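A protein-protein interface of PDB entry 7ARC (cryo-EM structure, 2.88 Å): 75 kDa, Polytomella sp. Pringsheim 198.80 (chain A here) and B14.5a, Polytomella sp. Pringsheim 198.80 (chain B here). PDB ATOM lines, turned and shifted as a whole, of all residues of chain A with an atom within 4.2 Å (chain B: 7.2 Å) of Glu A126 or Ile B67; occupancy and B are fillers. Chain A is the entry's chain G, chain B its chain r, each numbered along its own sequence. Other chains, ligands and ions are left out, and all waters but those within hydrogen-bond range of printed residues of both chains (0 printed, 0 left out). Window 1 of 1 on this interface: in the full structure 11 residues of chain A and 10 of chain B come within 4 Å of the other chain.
Of the printed residues of chain B, Glu A126 touches Ile B67 (3.99 Å), Lys B68 (3.5 Å), Tyr B69 (3.2 Å) and Phe B70 (3.1 Å). Of the printed residues of chain B, Glu A130 touches Ile B67 (3.3 Å). Lys B62 touches none of the printed residues of chain A. Of the printed residues of chain A, Leu B63 touches Arg A162. Of the printed residues of chain A, Asp B66 touches Arg A164. Of the printed residues of chain A, Ile B67 touches Glu A126 (3.99 Å), Glu A130 (3.3 Å), Ser A160 (3.2 Å), Arg A162 (3.3 Å) and Arg A164 (3.1 Å). Printed residues of chain A within 4 Å of Lys B68: Glu A126. Of the printed residues of chain A, Arg B72 touches Arg A162. The nearest printed residue of chain B that does not touch Glu A126 is Ala B71 (5.5 Å). The nearest printed residue of chain A that does not touch Tyr B69 is Ser A160 (4.2 Å).
Printed residues of chain B that touch a printed residue of chain A: Leu B63, Tyr B65, Asp B66, Ile B67, Lys B68, Tyr B69, Phe B70 and Arg B72. Printed residues of chain A that touch a printed residue of chain B: Lys A122, Lys A123, Glu A126, Glu A130, Ser A160, Arg A162 and Arg A164. Among the printed residues, 14 pairs touch across the chains. Among the printed residues, no Asp or Glu carboxylate lies within 4 Å of a Lys or Arg side-chain nitrogen of the other chain.
The side-chain hydroxyl (OG) of Ser A160 lies close to the backbone NH (N) of Arg A162 (3.4 Å). The guanidinium group (NE) of Arg A164 lies within salt-bridge range of the side-chain carboxylate (OE1) of Glu A130.
N of Tyr B69 lies within hydrogen-bond range of OE2 of Glu A126 (3.2 Å). The guanidinium group (NH2) of Arg A164 lies close to the backbone NH (N) of Ile B67 (3.1 Å). O of Tyr B65 sits close to NH2 of Arg A164, 3.0 Å away. The backbone NH (N) of Phe B70 sits at hydrogen-bond distance from the side-chain carboxylate (OE2) of Glu A126.
Among the printed residues, merely in contact across the chains: Lys A122 with Phe B70 (3.8 Å), Lys A123 with Phe B70 (3.8 Å), Glu A126 with Ile B67 (3.99 Å), Glu A126 with Lys B68 (3.5 Å), Glu A130 with Ile B67 (3.3 Å), Ser A160 with Ile B67 (3.2 Å), Arg A162 with Leu B63 (3.8 Å), Arg A162 with Ile B67 (3.3 Å), Arg A162 with Arg B72 (3.7 Å) and Arg A164 with Asp B66 (3.7 Å).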
ATOM      1  N   LYS A 122      20.982  24.614  37.823  1.00  0.00           N
ATOM      2  CA  LYS A 122      21.440  23.944  36.611  1.00  0.00           C
ATOM      3  C   LYS A 122      22.280  24.881  35.754  1.00  0.00           C
ATOM      4  O   LYS A 122      23.339  24.496  35.241  1.00  0.00           O
ATOM      5  CB  LYS A 122      20.242  23.422  35.821  1.00  0.00           C
ATOM      6  CG  LYS A 122      19.593  22.190  36.423  1.00  0.00           C
ATOM      7  CD  LYS A 122      18.363  21.776  35.639  1.00  0.00           C
ATOM      8  CE  LYS A 122      17.683  20.570  36.268  1.00  0.00           C
ATOM      9  NZ  LYS A 122      18.439  19.310  36.033  1.00  0.00           N
ATOM     10  N   LYS A 123      21.825  26.126  35.599  1.00  0.00           N
ATOM     11  CA  LYS A 123      22.577  27.100  34.817  1.00  0.00           C
ATOM     12  C   LYS A 123      23.921  27.415  35.472  1.00  0.00           C
ATOM     13  O   LYS A 123      24.941  27.538  34.784  1.00  0.00           O
ATOM     14  CB  LYS A 123      21.741  28.364  34.634  1.00  0.00           C
ATOM     15  CG  LYS A 123      22.386  29.436  33.783  1.00  0.00           C
ATOM     16  CD  LYS A 123      21.425  30.595  33.572  1.00  0.00           C
ATOM     17  CE  LYS A 123      22.093  31.744  32.846  1.00  0.00           C
ATOM     18  NZ  LYS A 123      22.459  31.365  31.454  1.00  0.00           N
ATOM     19  N   ALA A 124      23.937  27.558  36.799  1.00  0.00           N
ATOM     20  CA  ALA A 124      25.189  27.815  37.504  1.00  0.00           C
ATOM     21  C   ALA A 124      26.156  26.648  37.356  1.00  0.00           C
ATOM     22  O   ALA A 124      27.365  26.850  37.188  1.00  0.00           O
ATOM     23  CB  ALA A 124      24.913  28.097  38.979  1.00  0.00           C
ATOM     24  N   ARG A 125      25.643  25.419  37.430  1.00  0.00           N
ATOM     25  CA  ARG A 125      26.474  24.240  37.220  1.00  0.00           C
ATOM     26  C   ARG A 125      27.087  24.259  35.829  1.00  0.00           C
ATOM     27  O   ARG A 125      28.280  23.985  35.658  1.00  0.00           O
ATOM     28  CB  ARG A 125      25.649  22.972  37.418  1.00  0.00           C
ATOM     29  CG  ARG A 125      25.431  22.579  38.861  1.00  0.00           C
ATOM     30  CD  ARG A 125      24.317  21.560  38.964  1.00  0.00           C
ATOM     31  NE  ARG A 125      24.070  21.146  40.338  1.00  0.00           N
ATOM     32  CZ  ARG A 125      23.143  20.270  40.696  1.00  0.00           C
ATOM     33  NH1 ARG A 125      22.357  19.694  39.803  1.00  0.00           N
ATOM     34  NH2 ARG A 125      23.003  19.962  41.981  1.00  0.00           N
ATOM     35  N   GLU A 126      26.277  24.579  34.819  1.00  0.00           N
ATOM     36  CA  GLU A 126      26.790  24.618  33.455  1.00  0.00           C
ATOM     37  C   GLU A 126      27.855  25.696  33.298  1.00  0.00           C
ATOM     38  O   GLU A 126      28.869  25.485  32.621  1.00  0.00           O
ATOM     39  CB  GLU A 126      25.641  24.842  32.476  1.00  0.00           C
ATOM     40  CG  GLU A 126      24.760  23.626  32.296  1.00  0.00           C
ATOM     41  CD  GLU A 126      23.788  23.774  31.148  1.00  0.00           C
ATOM     42  OE1 GLU A 126      23.760  24.858  30.531  1.00  0.00           O
ATOM     43  OE2 GLU A 126      23.055  22.805  30.864  1.00  0.00           O
ATOM     44  N   GLY A 127      27.646  26.859  33.917  1.00  0.00           N
ATOM     45  CA  GLY A 127      28.637  27.920  33.821  1.00  0.00           C
ATOM     46  C   GLY A 127      29.948  27.564  34.498  1.00  0.00           C
ATOM     47  O   GLY A 127      31.030  27.821  33.958  1.00  0.00           O
ATOM     48  N   VAL A 128      29.872  26.968  35.691  1.00  0.00           N
ATOM     49  CA  VAL A 128      31.082  26.531  36.380  1.00  0.00           C
ATOM     50  C   VAL A 128      31.797  25.463  35.566  1.00  0.00           C
ATOM     51  O   VAL A 128      33.032  25.436  35.496  1.00  0.00           O
ATOM     52  CB  VAL A 128      30.744  26.038  37.799  1.00  0.00           C
ATOM     53  CG1 VAL A 128      31.969  25.431  38.451  1.00  0.00           C
ATOM     54  CG2 VAL A 128      30.225  27.181  38.640  1.00  0.00           C
ATOM     55  N   MET A 129      31.037  24.572  34.932  1.00  0.00           N
ATOM     56  CA  MET A 129      31.649  23.531  34.117  1.00  0.00           C
ATOM     57  C   MET A 129      32.364  24.136  32.913  1.00  0.00           C
ATOM     58  O   MET A 129      33.471  23.710  32.552  1.00  0.00           O
ATOM     59  CB  MET A 129      30.566  22.552  33.670  1.00  0.00           C
ATOM     60  CG  MET A 129      31.064  21.258  33.092  1.00  0.00           C
ATOM     61  SD  MET A 129      31.861  20.272  34.360  1.00  0.00           S
ATOM     62  CE  MET A 129      33.508  20.208  33.694  1.00  0.00           C
ATOM     63  N   GLU A 130      31.748  25.140  32.290  1.00  0.00           N
ATOM     64  CA  GLU A 130      32.389  25.855  31.193  1.00  0.00           C
ATOM     65  C   GLU A 130      33.696  26.497  31.637  1.00  0.00           C
ATOM     66  O   GLU A 130      34.724  26.383  30.957  1.00  0.00           O
ATOM     67  CB  GLU A 130      31.435  26.909  30.641  1.00  0.00           C
ATOM     68  CG  GLU A 130      31.893  27.549  29.356  1.00  0.00           C
ATOM     69  CD  GLU A 130      30.867  28.509  28.804  1.00  0.00           C
ATOM     70  OE1 GLU A 130      30.737  28.596  27.568  1.00  0.00           O
ATOM     71  OE2 GLU A 130      30.186  29.175  29.610  1.00  0.00           O
ATOM     72  N   PHE A 158      26.431  17.264  34.029  1.00  0.00           N
ATOM     73  CA  PHE A 158      26.067  18.598  34.497  1.00  0.00           C
ATOM     74  C   PHE A 158      26.650  19.701  33.622  1.00  0.00           C
ATOM     75  O   PHE A 158      26.896  20.808  34.101  1.00  0.00           O
ATOM     76  CB  PHE A 158      26.505  18.818  35.945  1.00  0.00           C
ATOM     77  CG  PHE A 158      26.152  17.699  36.872  1.00  0.00           C
ATOM     78  CD1 PHE A 158      24.882  17.603  37.405  1.00  0.00           C
ATOM     79  CD2 PHE A 158      27.098  16.757  37.233  1.00  0.00           C
ATOM     80  CE1 PHE A 158      24.555  16.582  38.269  1.00  0.00           C
ATOM     81  CE2 PHE A 158      26.778  15.733  38.097  1.00  0.00           C
ATOM     82  CZ  PHE A 158      25.505  15.645  38.616  1.00  0.00           C
ATOM     83  N   SER A 160      27.122  21.507  29.373  1.00  0.00           N
ATOM     84  CA  SER A 160      26.669  21.665  28.002  1.00  0.00           C
ATOM     85  C   SER A 160      27.512  20.823  27.049  1.00  0.00           C
ATOM     86  O   SER A 160      28.610  20.368  27.380  1.00  0.00           O
ATOM     87  CB  SER A 160      26.721  23.131  27.581  1.00  0.00           C
ATOM     88  OG  SER A 160      26.504  23.251  26.188  1.00  0.00           O
ATOM     89  N   ARG A 162      28.715  21.740  24.080  1.00  0.00           N
ATOM     90  CA  ARG A 162      29.410  22.567  23.105  1.00  0.00           C
ATOM     91  C   ARG A 162      30.121  23.695  23.831  1.00  0.00           C
ATOM     92  O   ARG A 162      29.802  24.025  24.976  1.00  0.00           O
ATOM     93  CB  ARG A 162      28.480  23.174  22.045  1.00  0.00           C
ATOM     94  CG  ARG A 162      27.849  22.212  21.067  1.00  0.00           C
ATOM     95  CD  ARG A 162      26.973  22.988  20.094  1.00  0.00           C
ATOM     96  NE  ARG A 162      26.345  22.138  19.093  1.00  0.00           N
ATOM     97  CZ  ARG A 162      25.157  21.570  19.229  1.00  0.00           C
ATOM     98  NH1 ARG A 162      24.440  21.723  20.329  1.00  0.00           N
ATOM     99  NH2 ARG A 162      24.679  20.826  18.237  1.00  0.00           N
ATOM    100  N   ARG A 164      32.182  27.691  23.537  1.00  0.00           N
ATOM    101  CA  ARG A 164      32.270  28.994  22.897  1.00  0.00           C
ATOM    102  C   ARG A 164      33.640  29.640  23.073  1.00  0.00           C
ATOM    103  O   ARG A 164      33.789  30.837  22.806  1.00  0.00           O
ATOM    104  CB  ARG A 164      31.162  29.893  23.451  1.00  0.00           C
ATOM    105  CG  ARG A 164      31.365  30.205  24.917  1.00  0.00           C
ATOM    106  CD  ARG A 164      30.244  31.020  25.538  1.00  0.00           C
ATOM    107  NE  ARG A 164      28.967  30.329  25.651  1.00  0.00           N
ATOM    108  CZ  ARG A 164      27.845  30.922  26.032  1.00  0.00           C
ATOM    109  NH1 ARG A 164      27.829  32.185  26.424  1.00  0.00           N
ATOM    110  NH2 ARG A 164      26.712  30.227  26.038  1.00  0.00           N
ATOM    111  N   LYS B  62      21.811  28.761  15.998  1.00  0.00           N
ATOM    112  CA  LYS B  62      21.804  29.593  17.193  1.00  0.00           C
ATOM    113  C   LYS B  62      22.365  28.883  18.417  1.00  0.00           C
ATOM    114  O   LYS B  62      22.217  29.393  19.532  1.00  0.00           O
ATOM    115  CB  LYS B  62      20.383  30.079  17.494  1.00  0.00           C
ATOM    116  CG  LYS B  62      19.767  30.946  16.414  1.00  0.00           C
ATOM    117  CD  LYS B  62      20.574  32.218  16.221  1.00  0.00           C
ATOM    118  CE  LYS B  62      20.493  33.112  17.450  1.00  0.00           C
ATOM    119  NZ  LYS B  62      19.115  33.616  17.697  1.00  0.00           N
ATOM    120  N   LEU B  63      23.000  27.727  18.242  1.00  0.00           N
ATOM    121  CA  LEU B  63      23.596  27.012  19.361  1.00  0.00           C
ATOM    122  C   LEU B  63      25.103  27.200  19.453  1.00  0.00           C
ATOM    123  O   LEU B  63      25.728  26.630  20.351  1.00  0.00           O
ATOM    124  CB  LEU B  63      23.267  25.518  19.263  1.00  0.00           C
ATOM    125  CG  LEU B  63      21.787  25.186  19.060  1.00  0.00           C
ATOM    126  CD1 LEU B  63      21.602  23.717  18.720  1.00  0.00           C
ATOM    127  CD2 LEU B  63      20.975  25.567  20.284  1.00  0.00           C
ATOM    128  N   VAL B  64      25.704  27.969  18.542  1.00  0.00           N
ATOM    129  CA  VAL B  64      27.157  28.100  18.534  1.00  0.00           C
ATOM    130  C   VAL B  64      27.635  28.801  19.800  1.00  0.00           C
ATOM    131  O   VAL B  64      28.495  28.293  20.528  1.00  0.00           O
ATOM    132  CB  VAL B  64      27.622  28.846  17.271  1.00  0.00           C
ATOM    133  CG1 VAL B  64      29.118  29.105  17.330  1.00  0.00           C
ATOM    134  CG2 VAL B  64      27.263  28.057  16.025  1.00  0.00           C
ATOM    135  N   TYR B  65      27.076  29.977  20.079  1.00  0.00           N
ATOM    136  CA  TYR B  65      27.491  30.799  21.205  1.00  0.00           C
ATOM    137  C   TYR B  65      26.473  30.832  22.334  1.00  0.00           C
ATOM    138  O   TYR B  65      26.685  31.548  23.317  1.00  0.00           O
ATOM    139  CB  TYR B  65      27.806  32.218  20.726  1.00  0.00           C
ATOM    140  CG  TYR B  65      29.138  32.302  20.017  1.00  0.00           C
ATOM    141  CD1 TYR B  65      29.267  32.984  18.822  1.00  0.00           C
ATOM    142  CD2 TYR B  65      30.268  31.699  20.548  1.00  0.00           C
ATOM    143  CE1 TYR B  65      30.477  33.064  18.167  1.00  0.00           C
ATOM    144  CE2 TYR B  65      31.488  31.773  19.904  1.00  0.00           C
ATOM    145  CZ  TYR B  65      31.585  32.457  18.713  1.00  0.00           C
ATOM    146  OH  TYR B  65      32.794  32.540  18.061  1.00  0.00           O
ATOM    147  N   ASP B  66      25.369  30.099  22.215  1.00  0.00           N
ATOM    148  CA  ASP B  66      24.335  30.061  23.245  1.00  0.00           C
ATOM    149  C   ASP B  66      24.149  28.606  23.655  1.00  0.00           C
ATOM    150  O   ASP B  66      23.394  27.863  23.018  1.00  0.00           O
ATOM    151  CB  ASP B  66      23.029  30.666  22.737  1.00  0.00           C
ATOM    152  CG  ASP B  66      22.025  30.903  23.848  1.00  0.00           C
ATOM    153  OD1 ASP B  66      22.351  31.643  24.797  1.00  0.00           O
ATOM    154  OD2 ASP B  66      20.907  30.349  23.773  1.00  0.00           O
ATOM    155  N   ILE B  67      24.830  28.204  24.723  1.00  0.00           N
ATOM    156  CA  ILE B  67      24.861  26.815  25.164  1.00  0.00           C
ATOM    157  C   ILE B  67      24.034  26.703  26.440  1.00  0.00           C
ATOM    158  O   ILE B  67      24.343  27.340  27.456  1.00  0.00           O
ATOM    159  CB  ILE B  67      26.301  26.303  25.345  1.00  0.00           C
ATOM    160  CG1 ILE B  67      27.062  27.075  26.425  1.00  0.00           C
ATOM    161  CG2 ILE B  67      27.054  26.390  24.025  1.00  0.00           C
ATOM    162  CD1 ILE B  67      28.394  26.460  26.795  1.00  0.00           C
ATOM    163  N   LYS B  68      22.943  25.944  26.371  1.00  0.00           N
ATOM    164  CA  LYS B  68      22.140  25.649  27.555  1.00  0.00           C
ATOM    165  C   LYS B  68      21.461  24.299  27.330  1.00  0.00           C
ATOM    166  O   LYS B  68      20.433  24.211  26.653  1.00  0.00           O
ATOM    167  CB  LYS B  68      21.156  26.782  27.846  1.00  0.00           C
ATOM    168  CG  LYS B  68      20.075  27.050  26.801  1.00  0.00           C
ATOM    169  CD  LYS B  68      19.163  28.187  27.224  1.00  0.00           C
ATOM    170  CE  LYS B  68      19.862  29.529  27.107  1.00  0.00           C
ATOM    171  NZ  LYS B  68      18.931  30.656  27.394  1.00  0.00           N
ATOM    172  N   TYR B  69      22.067  23.241  27.870  1.00  0.00           N
ATOM    173  CA  TYR B  69      21.512  21.912  27.650  1.00  0.00           C
ATOM    174  C   TYR B  69      20.267  21.668  28.494  1.00  0.00           C
ATOM    175  O   TYR B  69      19.311  21.047  28.018  1.00  0.00           O
ATOM    176  CB  TYR B  69      22.555  20.839  27.944  1.00  0.00           C
ATOM    177  CG  TYR B  69      22.108  19.468  27.504  1.00  0.00           C
ATOM    178  CD1 TYR B  69      21.758  19.227  26.184  1.00  0.00           C
ATOM    179  CD2 TYR B  69      21.983  18.431  28.414  1.00  0.00           C
ATOM    180  CE1 TYR B  69      21.335  17.981  25.774  1.00  0.00           C
ATOM    181  CE2 TYR B  69      21.551  17.183  28.016  1.00  0.00           C
ATOM    182  CZ  TYR B  69      21.232  16.962  26.694  1.00  0.00           C
ATOM    183  OH  TYR B  69      20.805  15.718  26.290  1.00  0.00           O
ATOM    184  N   PHE B  70      20.265  22.133  29.748  1.00  0.00           N
ATOM    185  CA  PHE B  70      19.133  21.879  30.636  1.00  0.00           C
ATOM    186  C   PHE B  70      17.824  22.399  30.054  1.00  0.00           C
ATOM    187  O   PHE B  70      16.758  21.834  30.320  1.00  0.00           O
ATOM    188  CB  PHE B  70      19.396  22.477  32.021  1.00  0.00           C
ATOM    189  CG  PHE B  70      19.361  23.976  32.062  1.00  0.00           C
ATOM    190  CD1 PHE B  70      20.412  24.724  31.563  1.00  0.00           C
ATOM    191  CD2 PHE B  70      18.281  24.638  32.617  1.00  0.00           C
ATOM    192  CE1 PHE B  70      20.384  26.101  31.606  1.00  0.00           C
ATOM    193  CE2 PHE B  70      18.247  26.016  32.663  1.00  0.00           C
ATOM    194  CZ  PHE B  70      19.301  26.748  32.158  1.00  0.00           C
ATOM    195  N   ALA B  71      17.885  23.466  29.257  1.00  0.00           N
ATOM    196  CA  ALA B  71      16.700  23.921  28.538  1.00  0.00           C
ATOM    197  C   ALA B  71      16.348  22.980  27.393  1.00  0.00           C
ATOM    198  O   ALA B  71      15.170  22.838  27.048  1.00  0.00           O
ATOM    199  CB  ALA B  71      16.914  25.341  28.017  1.00  0.00           C
ATOM    200  N   ARG B  72      17.350  22.345  26.788  1.00  0.00           N
ATOM    201  CA  ARG B  72      17.160  21.470  25.638  1.00  0.00           C
ATOM    202  C   ARG B  72      17.356  19.998  26.011  1.00  0.00           C
ATOM    203  O   ARG B  72      17.661  19.167  25.151  1.00  0.00           O
ATOM    204  CB  ARG B  72      18.127  21.906  24.530  1.00  0.00           C
ATOM    205  CG  ARG B  72      18.008  21.219  23.180  1.00  0.00           C
ATOM    206  CD  ARG B  72      19.041  21.776  22.219  1.00  0.00           C
ATOM    207  NE  ARG B  72      20.397  21.473  22.663  1.00  0.00           N
ATOM    208  CZ  ARG B  72      21.276  22.380  23.065  1.00  0.00           C
ATOM    209  NH1 ARG B  72      20.976  23.668  23.092  1.00  0.00           N
ATOM    210  NH2 ARG B  72      22.485  21.986  23.451  1.00  0.00           N
ATOM    211  N   ASP B  73      17.167  19.651  27.281  1.00  0.00           N
ATOM    212  CA  ASP B  73      17.365  18.283  27.761  1.00  0.00           C
ATOM    213  C   ASP B  73      16.006  17.606  27.895  1.00  0.00           C
ATOM    214  O   ASP B  73      15.288  17.816  28.875  1.00  0.00           O
ATOM    215  CB  ASP B  73      18.122  18.277  29.084  1.00  0.00           C
ATOM    216  CG  ASP B  73      18.153  16.907  29.728  1.00  0.00           C
ATOM    217  OD1 ASP B  73      18.639  15.956  29.084  1.00  0.00           O
ATOM    218  OD2 ASP B  73      17.692  16.781  30.881  1.00  0.00           O
